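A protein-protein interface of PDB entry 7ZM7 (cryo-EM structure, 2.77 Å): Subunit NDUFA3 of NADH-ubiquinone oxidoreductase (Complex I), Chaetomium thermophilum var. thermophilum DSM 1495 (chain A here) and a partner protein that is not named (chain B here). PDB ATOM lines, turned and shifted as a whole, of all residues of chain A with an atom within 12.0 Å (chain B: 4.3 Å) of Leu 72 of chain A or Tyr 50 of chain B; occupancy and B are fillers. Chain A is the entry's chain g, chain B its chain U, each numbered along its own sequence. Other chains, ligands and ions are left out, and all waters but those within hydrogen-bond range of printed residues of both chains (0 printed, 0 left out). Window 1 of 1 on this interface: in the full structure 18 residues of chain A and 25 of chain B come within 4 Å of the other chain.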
ATOM      1  N   TYR A  62     -44.904  13.560  23.412  1.00  0.00           N
ATOM      2  CA  TYR A  62     -43.768  13.966  22.553  1.00  0.00           C
ATOM      3  C   TYR A  62     -43.710  13.076  21.308  1.00  0.00           C
ATOM      4  O   TYR A  62     -43.721  11.851  21.471  1.00  0.00           O
ATOM      5  CB  TYR A  62     -42.420  14.050  23.276  1.00  0.00           C
ATOM      6  CG  TYR A  62     -41.315  14.580  22.399  1.00  0.00           C
ATOM      7  CD1 TYR A  62     -40.601  13.740  21.562  1.00  0.00           C
ATOM      8  CD2 TYR A  62     -41.004  15.927  22.374  1.00  0.00           C
ATOM      9  CE1 TYR A  62     -39.611  14.219  20.726  1.00  0.00           C
ATOM     10  CE2 TYR A  62     -40.001  16.422  21.559  1.00  0.00           C
ATOM     11  CZ  TYR A  62     -39.309  15.565  20.725  1.00  0.00           C
ATOM     12  OH  TYR A  62     -38.325  16.041  19.913  1.00  0.00           O
ATOM     13  N   PRO A  63     -43.606  13.633  20.068  1.00  0.00           N
ATOM     14  CA  PRO A  63     -43.639  12.780  18.900  1.00  0.00           C
ATOM     15  C   PRO A  63     -42.272  12.206  18.559  1.00  0.00           C
ATOM     16  O   PRO A  63     -41.555  12.819  17.797  1.00  0.00           O
ATOM     17  CB  PRO A  63     -44.057  13.761  17.827  1.00  0.00           C
ATOM     18  CG  PRO A  63     -43.461  15.077  18.255  1.00  0.00           C
ATOM     19  CD  PRO A  63     -43.526  15.051  19.759  1.00  0.00           C
ATOM     20  N   ILE A  64     -41.960  11.036  19.114  1.00  0.00           N
ATOM     21  CA  ILE A  64     -40.659  10.420  18.879  1.00  0.00           C
ATOM     22  C   ILE A  64     -40.653   9.711  17.533  1.00  0.00           C
ATOM     23  O   ILE A  64     -41.543   8.891  17.262  1.00  0.00           O
ATOM     24  CB  ILE A  64     -40.304   9.472  20.025  1.00  0.00           C
ATOM     25  CG1 ILE A  64     -40.049  10.310  21.279  1.00  0.00           C
ATOM     26  CG2 ILE A  64     -39.109   8.621  19.665  1.00  0.00           C
ATOM     27  CD1 ILE A  64     -40.315   9.647  22.546  1.00  0.00           C
ATOM     28  N   PRO A  65     -39.687   9.988  16.665  1.00  0.00           N
ATOM     29  CA  PRO A  65     -39.647   9.320  15.379  1.00  0.00           C
ATOM     30  C   PRO A  65     -39.043   7.933  15.489  1.00  0.00           C
ATOM     31  O   PRO A  65     -38.182   7.676  16.344  1.00  0.00           O
ATOM     32  CB  PRO A  65     -38.777  10.264  14.534  1.00  0.00           C
ATOM     33  CG  PRO A  65     -37.997  11.115  15.578  1.00  0.00           C
ATOM     34  CD  PRO A  65     -38.378  10.594  16.933  1.00  0.00           C
ATOM     35  N   PRO A  66     -39.483   7.003  14.650  1.00  0.00           N
ATOM     36  CA  PRO A  66     -38.969   5.636  14.705  1.00  0.00           C
ATOM     37  C   PRO A  66     -37.694   5.468  13.898  1.00  0.00           C
ATOM     38  O   PRO A  66     -37.391   6.235  12.985  1.00  0.00           O
ATOM     39  CB  PRO A  66     -40.115   4.821  14.091  1.00  0.00           C
ATOM     40  CG  PRO A  66     -40.737   5.758  13.111  1.00  0.00           C
ATOM     41  CD  PRO A  66     -40.508   7.167  13.606  1.00  0.00           C
ATOM     42  N   GLY A  67     -36.940   4.436  14.260  1.00  0.00           N
ATOM     43  CA  GLY A  67     -35.704   4.125  13.586  1.00  0.00           C
ATOM     44  C   GLY A  67     -34.501   4.374  14.467  1.00  0.00           C
ATOM     45  O   GLY A  67     -34.621   4.840  15.603  1.00  0.00           O
ATOM     46  N   PRO A  68     -33.313   4.061  13.960  1.00  0.00           N
ATOM     47  CA  PRO A  68     -32.096   4.288  14.741  1.00  0.00           C
ATOM     48  C   PRO A  68     -31.783   5.770  14.865  1.00  0.00           C
ATOM     49  O   PRO A  68     -32.212   6.596  14.057  1.00  0.00           O
ATOM     50  CB  PRO A  68     -31.019   3.561  13.932  1.00  0.00           C
ATOM     51  CG  PRO A  68     -31.526   3.609  12.535  1.00  0.00           C
ATOM     52  CD  PRO A  68     -33.022   3.495  12.633  1.00  0.00           C
ATOM     53  N   ARG A  69     -31.015   6.094  15.901  1.00  0.00           N
ATOM     54  CA  ARG A  69     -30.574   7.461  16.119  1.00  0.00           C
ATOM     55  C   ARG A  69     -29.660   7.914  14.984  1.00  0.00           C
ATOM     56  O   ARG A  69     -28.940   7.117  14.380  1.00  0.00           O
ATOM     57  CB  ARG A  69     -29.859   7.569  17.460  1.00  0.00           C
ATOM     58  CG  ARG A  69     -30.775   7.432  18.665  1.00  0.00           C
ATOM     59  CD  ARG A  69     -29.989   7.460  19.947  1.00  0.00           C
ATOM     60  NE  ARG A  69     -29.294   8.724  20.138  1.00  0.00           N
ATOM     61  CZ  ARG A  69     -28.408   8.946  21.097  1.00  0.00           C
ATOM     62  NH1 ARG A  69     -27.824  10.124  21.204  1.00  0.00           N
ATOM     63  NH2 ARG A  69     -28.109   7.986  21.953  1.00  0.00           N
ATOM     64  N   LYS A  70     -29.699   9.212  14.694  1.00  0.00           N
ATOM     65  CA  LYS A  70     -29.149   9.748  13.456  1.00  0.00           C
ATOM     66  C   LYS A  70     -27.655  10.016  13.500  1.00  0.00           C
ATOM     67  O   LYS A  70     -27.084  10.362  12.461  1.00  0.00           O
ATOM     68  CB  LYS A  70     -29.866  11.045  13.073  1.00  0.00           C
ATOM     69  CG  LYS A  70     -31.255  10.861  12.508  1.00  0.00           C
ATOM     70  CD  LYS A  70     -31.785  12.179  11.984  1.00  0.00           C
ATOM     71  CE  LYS A  70     -33.156  12.016  11.365  1.00  0.00           C
ATOM     72  NZ  LYS A  70     -33.624  13.288  10.757  1.00  0.00           N
ATOM     73  N   GLN A  71     -27.011   9.885  14.657  1.00  0.00           N
ATOM     74  CA  GLN A  71     -25.577  10.149  14.790  1.00  0.00           C
ATOM     75  C   GLN A  71     -25.245  11.587  14.384  1.00  0.00           C
ATOM     76  O   GLN A  71     -24.579  11.846  13.380  1.00  0.00           O
ATOM     77  CB  GLN A  71     -24.759   9.139  13.978  1.00  0.00           C
ATOM     78  CG  GLN A  71     -23.292   9.081  14.350  1.00  0.00           C
ATOM     79  CD  GLN A  71     -22.430   8.600  13.206  1.00  0.00           C
ATOM     80  OE1 GLN A  71     -22.937   8.214  12.155  1.00  0.00           O
ATOM     81  NE2 GLN A  71     -21.118   8.620  13.404  1.00  0.00           N
ATOM     82  N   LEU A  72     -25.744  12.525  15.182  1.00  0.00           N
ATOM     83  CA  LEU A  72     -25.531  13.940  14.918  1.00  0.00           C
ATOM     84  C   LEU A  72     -24.084  14.344  15.161  1.00  0.00           C
ATOM     85  O   LEU A  72     -23.345  13.693  15.904  1.00  0.00           O
ATOM     86  CB  LEU A  72     -26.441  14.797  15.799  1.00  0.00           C
ATOM     87  CG  LEU A  72     -27.805  15.197  15.246  1.00  0.00           C
ATOM     88  CD1 LEU A  72     -27.619  16.079  14.029  1.00  0.00           C
ATOM     89  CD2 LEU A  72     -28.618  13.969  14.903  1.00  0.00           C
ATOM     90  N   LYS A  73     -23.688  15.438  14.515  1.00  0.00           N
ATOM     91  CA  LYS A  73     -22.409  16.091  14.742  1.00  0.00           C
ATOM     92  C   LYS A  73     -22.622  17.592  14.674  1.00  0.00           C
ATOM     93  O   LYS A  73     -23.145  18.102  13.678  1.00  0.00           O
ATOM     94  CB  LYS A  73     -21.362  15.660  13.710  1.00  0.00           C
ATOM     95  CG  LYS A  73     -20.863  14.240  13.887  1.00  0.00           C
ATOM     96  CD  LYS A  73     -20.178  14.067  15.229  1.00  0.00           C
ATOM     97  CE  LYS A  73     -18.896  14.876  15.295  1.00  0.00           C
ATOM     98  NZ  LYS A  73     -17.917  14.426  14.268  1.00  0.00           N
ATOM     99  N   GLY A  74     -22.314  18.296  15.767  1.00  0.00           N
ATOM    100  CA  GLY A  74     -22.559  19.748  15.864  1.00  0.00           C
ATOM    101  C   GLY A  74     -22.805  20.187  17.282  1.00  0.00           C
ATOM    102  O   GLY A  74     -23.097  19.308  18.107  1.00  0.00           O
ATOM    103  N   TYR A  75     -22.702  21.486  17.563  1.00  0.00           N
ATOM    104  CA  TYR A  75     -23.107  21.993  18.895  1.00  0.00           C
ATOM    105  C   TYR A  75     -22.433  21.193  20.013  1.00  0.00           C
ATOM    106  O   TYR A  75     -23.097  20.824  20.990  1.00  0.00           O
ATOM    107  CB  TYR A  75     -24.633  22.057  18.964  1.00  0.00           C
ATOM    108  CG  TYR A  75     -25.267  22.991  17.969  1.00  0.00           C
ATOM    109  CD1 TYR A  75     -25.079  24.359  18.058  1.00  0.00           C
ATOM    110  CD2 TYR A  75     -26.060  22.508  16.945  1.00  0.00           C
ATOM    111  CE1 TYR A  75     -25.656  25.224  17.147  1.00  0.00           C
ATOM    112  CE2 TYR A  75     -26.647  23.359  16.027  1.00  0.00           C
ATOM    113  CZ  TYR A  75     -26.444  24.723  16.129  1.00  0.00           C
ATOM    114  OH  TYR A  75     -27.019  25.571  15.229  1.00  0.00           O
ATOM    115  N   ASP A  76     -21.125  20.969  19.898  1.00  0.00           N
ATOM    116  CA  ASP A  76     -20.436  20.124  20.907  1.00  0.00           C
ATOM    117  C   ASP A  76     -19.852  20.990  22.026  1.00  0.00           C
ATOM    118  O   ASP A  76     -20.009  22.217  21.965  1.00  0.00           O
ATOM    119  CB  ASP A  76     -19.408  19.196  20.259  1.00  0.00           C
ATOM    120  CG  ASP A  76     -19.979  17.829  19.927  1.00  0.00           C
ATOM    121  OD1 ASP A  76     -21.102  17.543  20.384  1.00  0.00           O
ATOM    122  OD2 ASP A  76     -19.297  17.064  19.220  1.00  0.00           O
ATOM    123  N   ASP A  77     -19.208  20.360  23.009  1.00  0.00           N
ATOM    124  CA  ASP A  77     -18.667  21.093  24.183  1.00  0.00           C
ATOM    125  C   ASP A  77     -17.638  22.129  23.717  1.00  0.00           C
ATOM    126  O   ASP A  77     -17.574  23.206  24.330  1.00  0.00           O
ATOM    127  CB  ASP A  77     -18.075  20.121  25.206  1.00  0.00           C
ATOM    128  CG  ASP A  77     -19.091  19.134  25.754  1.00  0.00           C
ATOM    129  OD1 ASP A  77     -20.191  19.575  26.128  1.00  0.00           O
ATOM    130  OD2 ASP A  77     -18.773  17.929  25.794  1.00  0.00           O
ATOM    131  N   ASP A  78     -16.850  21.799  22.693  1.00  0.00           N
ATOM    132  CA  ASP A  78     -15.834  22.749  22.170  1.00  0.00           C
ATOM    133  C   ASP A  78     -16.527  24.016  21.650  1.00  0.00           C
ATOM    134  O   ASP A  78     -15.986  25.114  21.885  1.00  0.00           O
ATOM    135  CB  ASP A  78     -14.913  22.085  21.141  1.00  0.00           C
ATOM    136  CG  ASP A  78     -15.625  21.186  20.144  1.00  0.00           C
ATOM    137  OD1 ASP A  78     -16.844  21.357  19.958  1.00  0.00           O
ATOM    138  OD2 ASP A  78     -14.950  20.316  19.561  1.00  0.00           O
ATOM    139  N   THR A  79     -17.671  23.874  20.975  1.00  0.00           N
ATOM    140  CA  THR A  79     -18.401  25.044  20.413  1.00  0.00           C
ATOM    141  C   THR A  79     -18.879  25.969  21.539  1.00  0.00           C
ATOM    142  O   THR A  79     -18.817  27.194  21.328  1.00  0.00           O
ATOM    143  CB  THR A  79     -19.551  24.615  19.493  1.00  0.00           C
ATOM    144  OG1 THR A  79     -20.662  24.199  20.289  1.00  0.00           O
ATOM    145  CG2 THR A  79     -19.158  23.521  18.524  1.00  0.00           C
ATOM    146  N   GLU A  80     -19.351  25.408  22.660  1.00  0.00           N
ATOM    147  CA  GLU A  80     -19.875  26.212  23.804  1.00  0.00           C
ATOM    148  C   GLU A  80     -19.296  27.630  23.768  1.00  0.00           C
ATOM    149  O   GLU A  80     -18.247  27.833  24.410  1.00  0.00           O
ATOM    150  CB  GLU A  80     -19.513  25.540  25.128  1.00  0.00           C
ATOM    151  CG  GLU A  80     -20.660  25.448  26.117  1.00  0.00           C
ATOM    152  CD  GLU A  80     -21.077  26.752  26.768  1.00  0.00           C
ATOM    153  OE1 GLU A  80     -20.186  27.540  27.140  1.00  0.00           O
ATOM    154  OE2 GLU A  80     -22.291  26.977  26.894  1.00  0.00           O
ATOM    155  N   CYS B  47     -33.229  22.792  15.250  1.00  0.00           N
ATOM    156  CA  CYS B  47     -32.684  21.853  16.251  1.00  0.00           C
ATOM    157  C   CYS B  47     -33.508  20.593  16.345  1.00  0.00           C
ATOM    158  O   CYS B  47     -33.293  19.846  17.281  1.00  0.00           O
ATOM    159  CB  CYS B  47     -32.803  22.529  17.598  1.00  0.00           C
ATOM    160  SG  CYS B  47     -32.160  24.212  17.507  1.00  0.00           S
ATOM    161  N   LYS B  48     -34.345  20.333  15.359  1.00  0.00           N
ATOM    162  CA  LYS B  48     -35.256  19.192  15.503  1.00  0.00           C
ATOM    163  C   LYS B  48     -34.429  17.933  15.659  1.00  0.00           C
ATOM    164  O   LYS B  48     -34.829  17.090  16.440  1.00  0.00           O
ATOM    165  CB  LYS B  48     -36.141  19.126  14.264  1.00  0.00           C
ATOM    166  CG  LYS B  48     -37.399  18.279  14.388  1.00  0.00           C
ATOM    167  CD  LYS B  48     -38.253  18.294  13.141  1.00  0.00           C
ATOM    168  CE  LYS B  48     -37.490  17.917  11.888  1.00  0.00           C
ATOM    169  NZ  LYS B  48     -37.043  19.108  11.127  1.00  0.00           N
ATOM    170  N   ASP B  49     -33.338  17.810  14.917  1.00  0.00           N
ATOM    171  CA  ASP B  49     -32.501  16.588  14.941  1.00  0.00           C
ATOM    172  C   ASP B  49     -31.895  16.391  16.312  1.00  0.00           C
ATOM    173  O   ASP B  49     -31.936  15.266  16.801  1.00  0.00           O
ATOM    174  CB  ASP B  49     -31.348  16.728  13.959  1.00  0.00           C
ATOM    175  CG  ASP B  49     -31.769  16.464  12.522  1.00  0.00           C
ATOM    176  OD1 ASP B  49     -32.974  16.227  12.301  1.00  0.00           O
ATOM    177  OD2 ASP B  49     -30.891  16.491  11.637  1.00  0.00           O
ATOM    178  N   TYR B  50     -31.444  17.479  16.919  1.00  0.00           N
ATOM    179  CA  TYR B  50     -30.793  17.457  18.243  1.00  0.00           C
ATOM    180  C   TYR B  50     -31.889  17.226  19.277  1.00  0.00           C
ATOM    181  O   TYR B  50     -31.690  16.443  20.189  1.00  0.00           O
ATOM    182  CB  TYR B  50     -30.037  18.769  18.374  1.00  0.00           C
ATOM    183  CG  TYR B  50     -28.921  18.956  17.378  1.00  0.00           C
ATOM    184  CD1 TYR B  50     -27.661  18.438  17.619  1.00  0.00           C
ATOM    185  CD2 TYR B  50     -29.119  19.663  16.208  1.00  0.00           C
ATOM    186  CE1 TYR B  50     -26.627  18.608  16.715  1.00  0.00           C
ATOM    187  CE2 TYR B  50     -28.098  19.837  15.291  1.00  0.00           C
ATOM    188  CZ  TYR B  50     -26.847  19.307  15.545  1.00  0.00           C
ATOM    189  OH  TYR B  50     -25.837  19.477  14.646  1.00  0.00           O
ATOM    190  N   ASN B  51     -33.034  17.872  19.089  1.00  0.00           N
ATOM    191  CA  ASN B  51     -34.192  17.752  20.012  1.00  0.00           C
ATOM    192  C   ASN B  51     -34.709  16.319  19.984  1.00  0.00           C
ATOM    193  O   ASN B  51     -35.144  15.843  21.030  1.00  0.00           O
ATOM    194  CB  ASN B  51     -35.296  18.769  19.698  1.00  0.00           C
ATOM    195  CG  ASN B  51     -34.970  20.208  20.015  1.00  0.00           C
ATOM    196  OD1 ASN B  51     -33.901  20.514  20.528  1.00  0.00           O
ATOM    197  ND2 ASN B  51     -35.897  21.099  19.710  1.00  0.00           N
ATOM    198  N   ASP B  52     -34.663  15.674  18.829  1.00  0.00           N
ATOM    199  CA  ASP B  52     -35.225  14.311  18.680  1.00  0.00           C
ATOM    200  C   ASP B  52     -34.184  13.300  19.128  1.00  0.00           C
ATOM    201  O   ASP B  52     -34.571  12.295  19.727  1.00  0.00           O
ATOM    202  CB  ASP B  52     -35.678  14.108  17.236  1.00  0.00           C
ATOM    203  CG  ASP B  52     -37.114  14.527  16.995  1.00  0.00           C
ATOM    204  OD1 ASP B  52     -37.977  14.133  17.798  1.00  0.00           O
ATOM    205  OD2 ASP B  52     -37.355  15.247  16.009  1.00  0.00           O
ATOM    206  N   ASP B  53     -32.902  13.607  18.925  1.00  0.00           N
ATOM    207  CA  ASP B  53     -31.809  12.716  19.379  1.00  0.00           C
ATOM    208  C   ASP B  53     -31.814  12.671  20.904  1.00  0.00           C
ATOM    209  O   ASP B  53     -31.643  11.580  21.462  1.00  0.00           O
ATOM    210  CB  ASP B  53     -30.461  13.208  18.868  1.00  0.00           C
ATOM    211  CG  ASP B  53     -29.324  12.234  19.092  1.00  0.00           C
ATOM    212  OD1 ASP B  53     -29.514  11.045  18.799  1.00  0.00           O
ATOM    213  OD2 ASP B  53     -28.262  12.681  19.556  1.00  0.00           O
ATOM    214  N   TYR B  54     -31.999  13.820  21.545  1.00  0.00           N
ATOM    215  CA  TYR B  54     -31.975  13.890  23.026  1.00  0.00           C
ATOM    216  C   TYR B  54     -33.112  13.058  23.591  1.00  0.00           C
ATOM    217  O   TYR B  54     -32.923  12.399  24.614  1.00  0.00           O
ATOM    218  CB  TYR B  54     -32.083  15.332  23.511  1.00  0.00           C
ATOM    219  CG  TYR B  54     -32.293  15.492  24.994  1.00  0.00           C
ATOM    220  CD1 TYR B  54     -31.290  15.180  25.894  1.00  0.00           C
ATOM    221  CD2 TYR B  54     -33.497  15.950  25.494  1.00  0.00           C
ATOM    222  CE1 TYR B  54     -31.476  15.321  27.256  1.00  0.00           C
ATOM    223  CE2 TYR B  54     -33.702  16.100  26.854  1.00  0.00           C
ATOM    224  CZ  TYR B  54     -32.688  15.782  27.736  1.00  0.00           C
ATOM    225  OH  TYR B  54     -32.882  15.930  29.075  1.00  0.00           O
ATOM    226  N   ARG B  75     -26.113  19.631  23.809  1.00  0.00           N
ATOM    227  CA  ARG B  75     -26.235  19.904  22.360  1.00  0.00           C
ATOM    228  C   ARG B  75     -27.537  20.657  22.049  1.00  0.00           C
ATOM    229  O   ARG B  75     -27.487  21.594  21.254  1.00  0.00           O
ATOM    230  CB  ARG B  75     -26.074  18.614  21.551  1.00  0.00           C
ATOM    231  CG  ARG B  75     -24.707  17.961  21.637  1.00  0.00           C
ATOM    232  CD  ARG B  75     -24.776  16.687  20.826  1.00  0.00           C
ATOM    233  NE  ARG B  75     -23.539  15.924  20.817  1.00  0.00           N
ATOM    234  CZ  ARG B  75     -23.380  14.784  20.160  1.00  0.00           C
ATOM    235  NH1 ARG B  75     -22.221  14.151  20.201  1.00  0.00           N
ATOM    236  NH2 ARG B  75     -24.381  14.281  19.460  1.00  0.00           N
ATOM    237  N   VAL B  76     -28.654  20.286  22.673  1.00  0.00           N
ATOM    238  CA  VAL B  76     -29.952  20.996  22.444  1.00  0.00           C
ATOM    239  C   VAL B  76     -29.900  22.451  22.933  1.00  0.00           C
ATOM    240  O   VAL B  76     -30.395  23.313  22.215  1.00  0.00           O
ATOM    241  CB  VAL B  76     -31.195  20.230  22.954  1.00  0.00           C
ATOM    242  CG1 VAL B  76     -31.131  18.751  22.633  1.00  0.00           C
ATOM    243  CG2 VAL B  76     -31.501  20.452  24.422  1.00  0.00           C
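The side-chain hydroxyl of Tyr 62 of chain A is in hydrogen-bond range of the backbone carbonyl oxygen of Asn 51 of chain B. OD1 of Asp 53 of chain B lies within salt-bridge range of NE of Arg 69 of chain A, at 2.7 Å. OD1 of Asp 49 of chain B is in salt-bridge range of NZ of Lys 70 of chain A. OD1 of Asp 76 of chain A lies within salt-bridge range of NE of Arg 75 of chain B, 3.0 Å away. OD1 of Asp 52 of chain B lies within hydrogen-bond range of OH of Tyr 62 of chain A, 2.9 Å away. The backbone carbonyl oxygen (O) of Lys 73 of chain A lies within hydrogen-bond range of the side-chain hydroxyl (OH) of Tyr 50 of chain B.
The side-chain hydroxyl (OG1) of Thr 79 of chain A lies within hydrogen-bond range of the backbone carbonyl oxygen (O) of Asp 76 of chain A. O of Cys 47 of chain B sits close to OD1 of Asn 51 of chain B, at 3.4 Å.
Pro 63 of chain A touches Asp 52 of chain B. Asp 52 of chain B touches Pro 65 of chain A. Asp 49 of chain B touches Leu 72 of chain A. Leu 72 of chain A touches Tyr 50 of chain B (CD1 to CZ, 3.6 Å). Arg 75 of chain B touches Leu 72 of chain A. Gly 74 of chain A touches Tyr 50 of chain B (CA to OH, 3.5 Å). Tyr 50 of chain B touches Tyr 75 of chain A (CZ to CD2, 3.6 Å). Arg 75 of chain B touches Tyr 75 of chain A (CG to O, 3.3 Å).
Printed residues of chain B within 4 Å of Tyr 62 of chain A: Asn 51 (3.4 Å) and Asp 52 (2.9 Å). Of the printed residues of chain B, Arg 69 of chain A touches Asp 53 (2.7 Å). Printed residues of chain B within 4 Å of Lys 70 of chain A: Asp 49 (3.4 Å). Printed residues of chain B within 4 Å of Leu 72 of chain A: Asp 49, Tyr 50 and Arg 75. Printed residues of chain B within 4 Å of Tyr 75 of chain A: Tyr 50 (3.6 Å) and Arg 75 (3.3 Å). Of the printed residues of chain B, Asp 76 of chain A touches Arg 75 (3.0 Å). No residue of chain A comes within 4 Å of Cys 47 of chain B. Asp 49 of chain B touches just these residues of chain A: Lys 70 (3.4 Å) and Leu 72 (3.8 Å). Of chain A, only Leu 72 (3.6 Å), Lys 73 (3.2 Å), Gly 74 (3.5 Å) and Tyr 75 (3.6 Å) come within 4 Å of Tyr 50 of chain B. Printed residues of chain A within 4 Å of Asn 51 of chain B: Tyr 62 (3.4 Å). Of the printed residues of chain A, Asp 52 of chain B touches Tyr 62 (2.9 Å), Pro 63 (3.8 Å) and Pro 65 (3.7 Å). Asp 53 of chain B touches just one residue of chain A: Arg 69. No residue of chain A comes within 4 Å of Val 76 of chain B. The nearest printed residue of chain B that does not touch Leu 72 of chain A is Asp 53 of chain B (4.4 Å). The nearest residue of chain A that does not touch Tyr 50 of chain B is Tyr 62 of chain A (6.6 Å). The nearest printed residue of chain B that does not touch Pro 65 of chain A is Asp 53 of chain B (6.6 Å).
Of the 10 printed residues of chain B, 6 touch a printed residue of chain A. Hydrophobic or aromatic side chains of chain A that line the printed part of chain B: Tyr 62, Pro 65, Leu 72 and Tyr 75.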
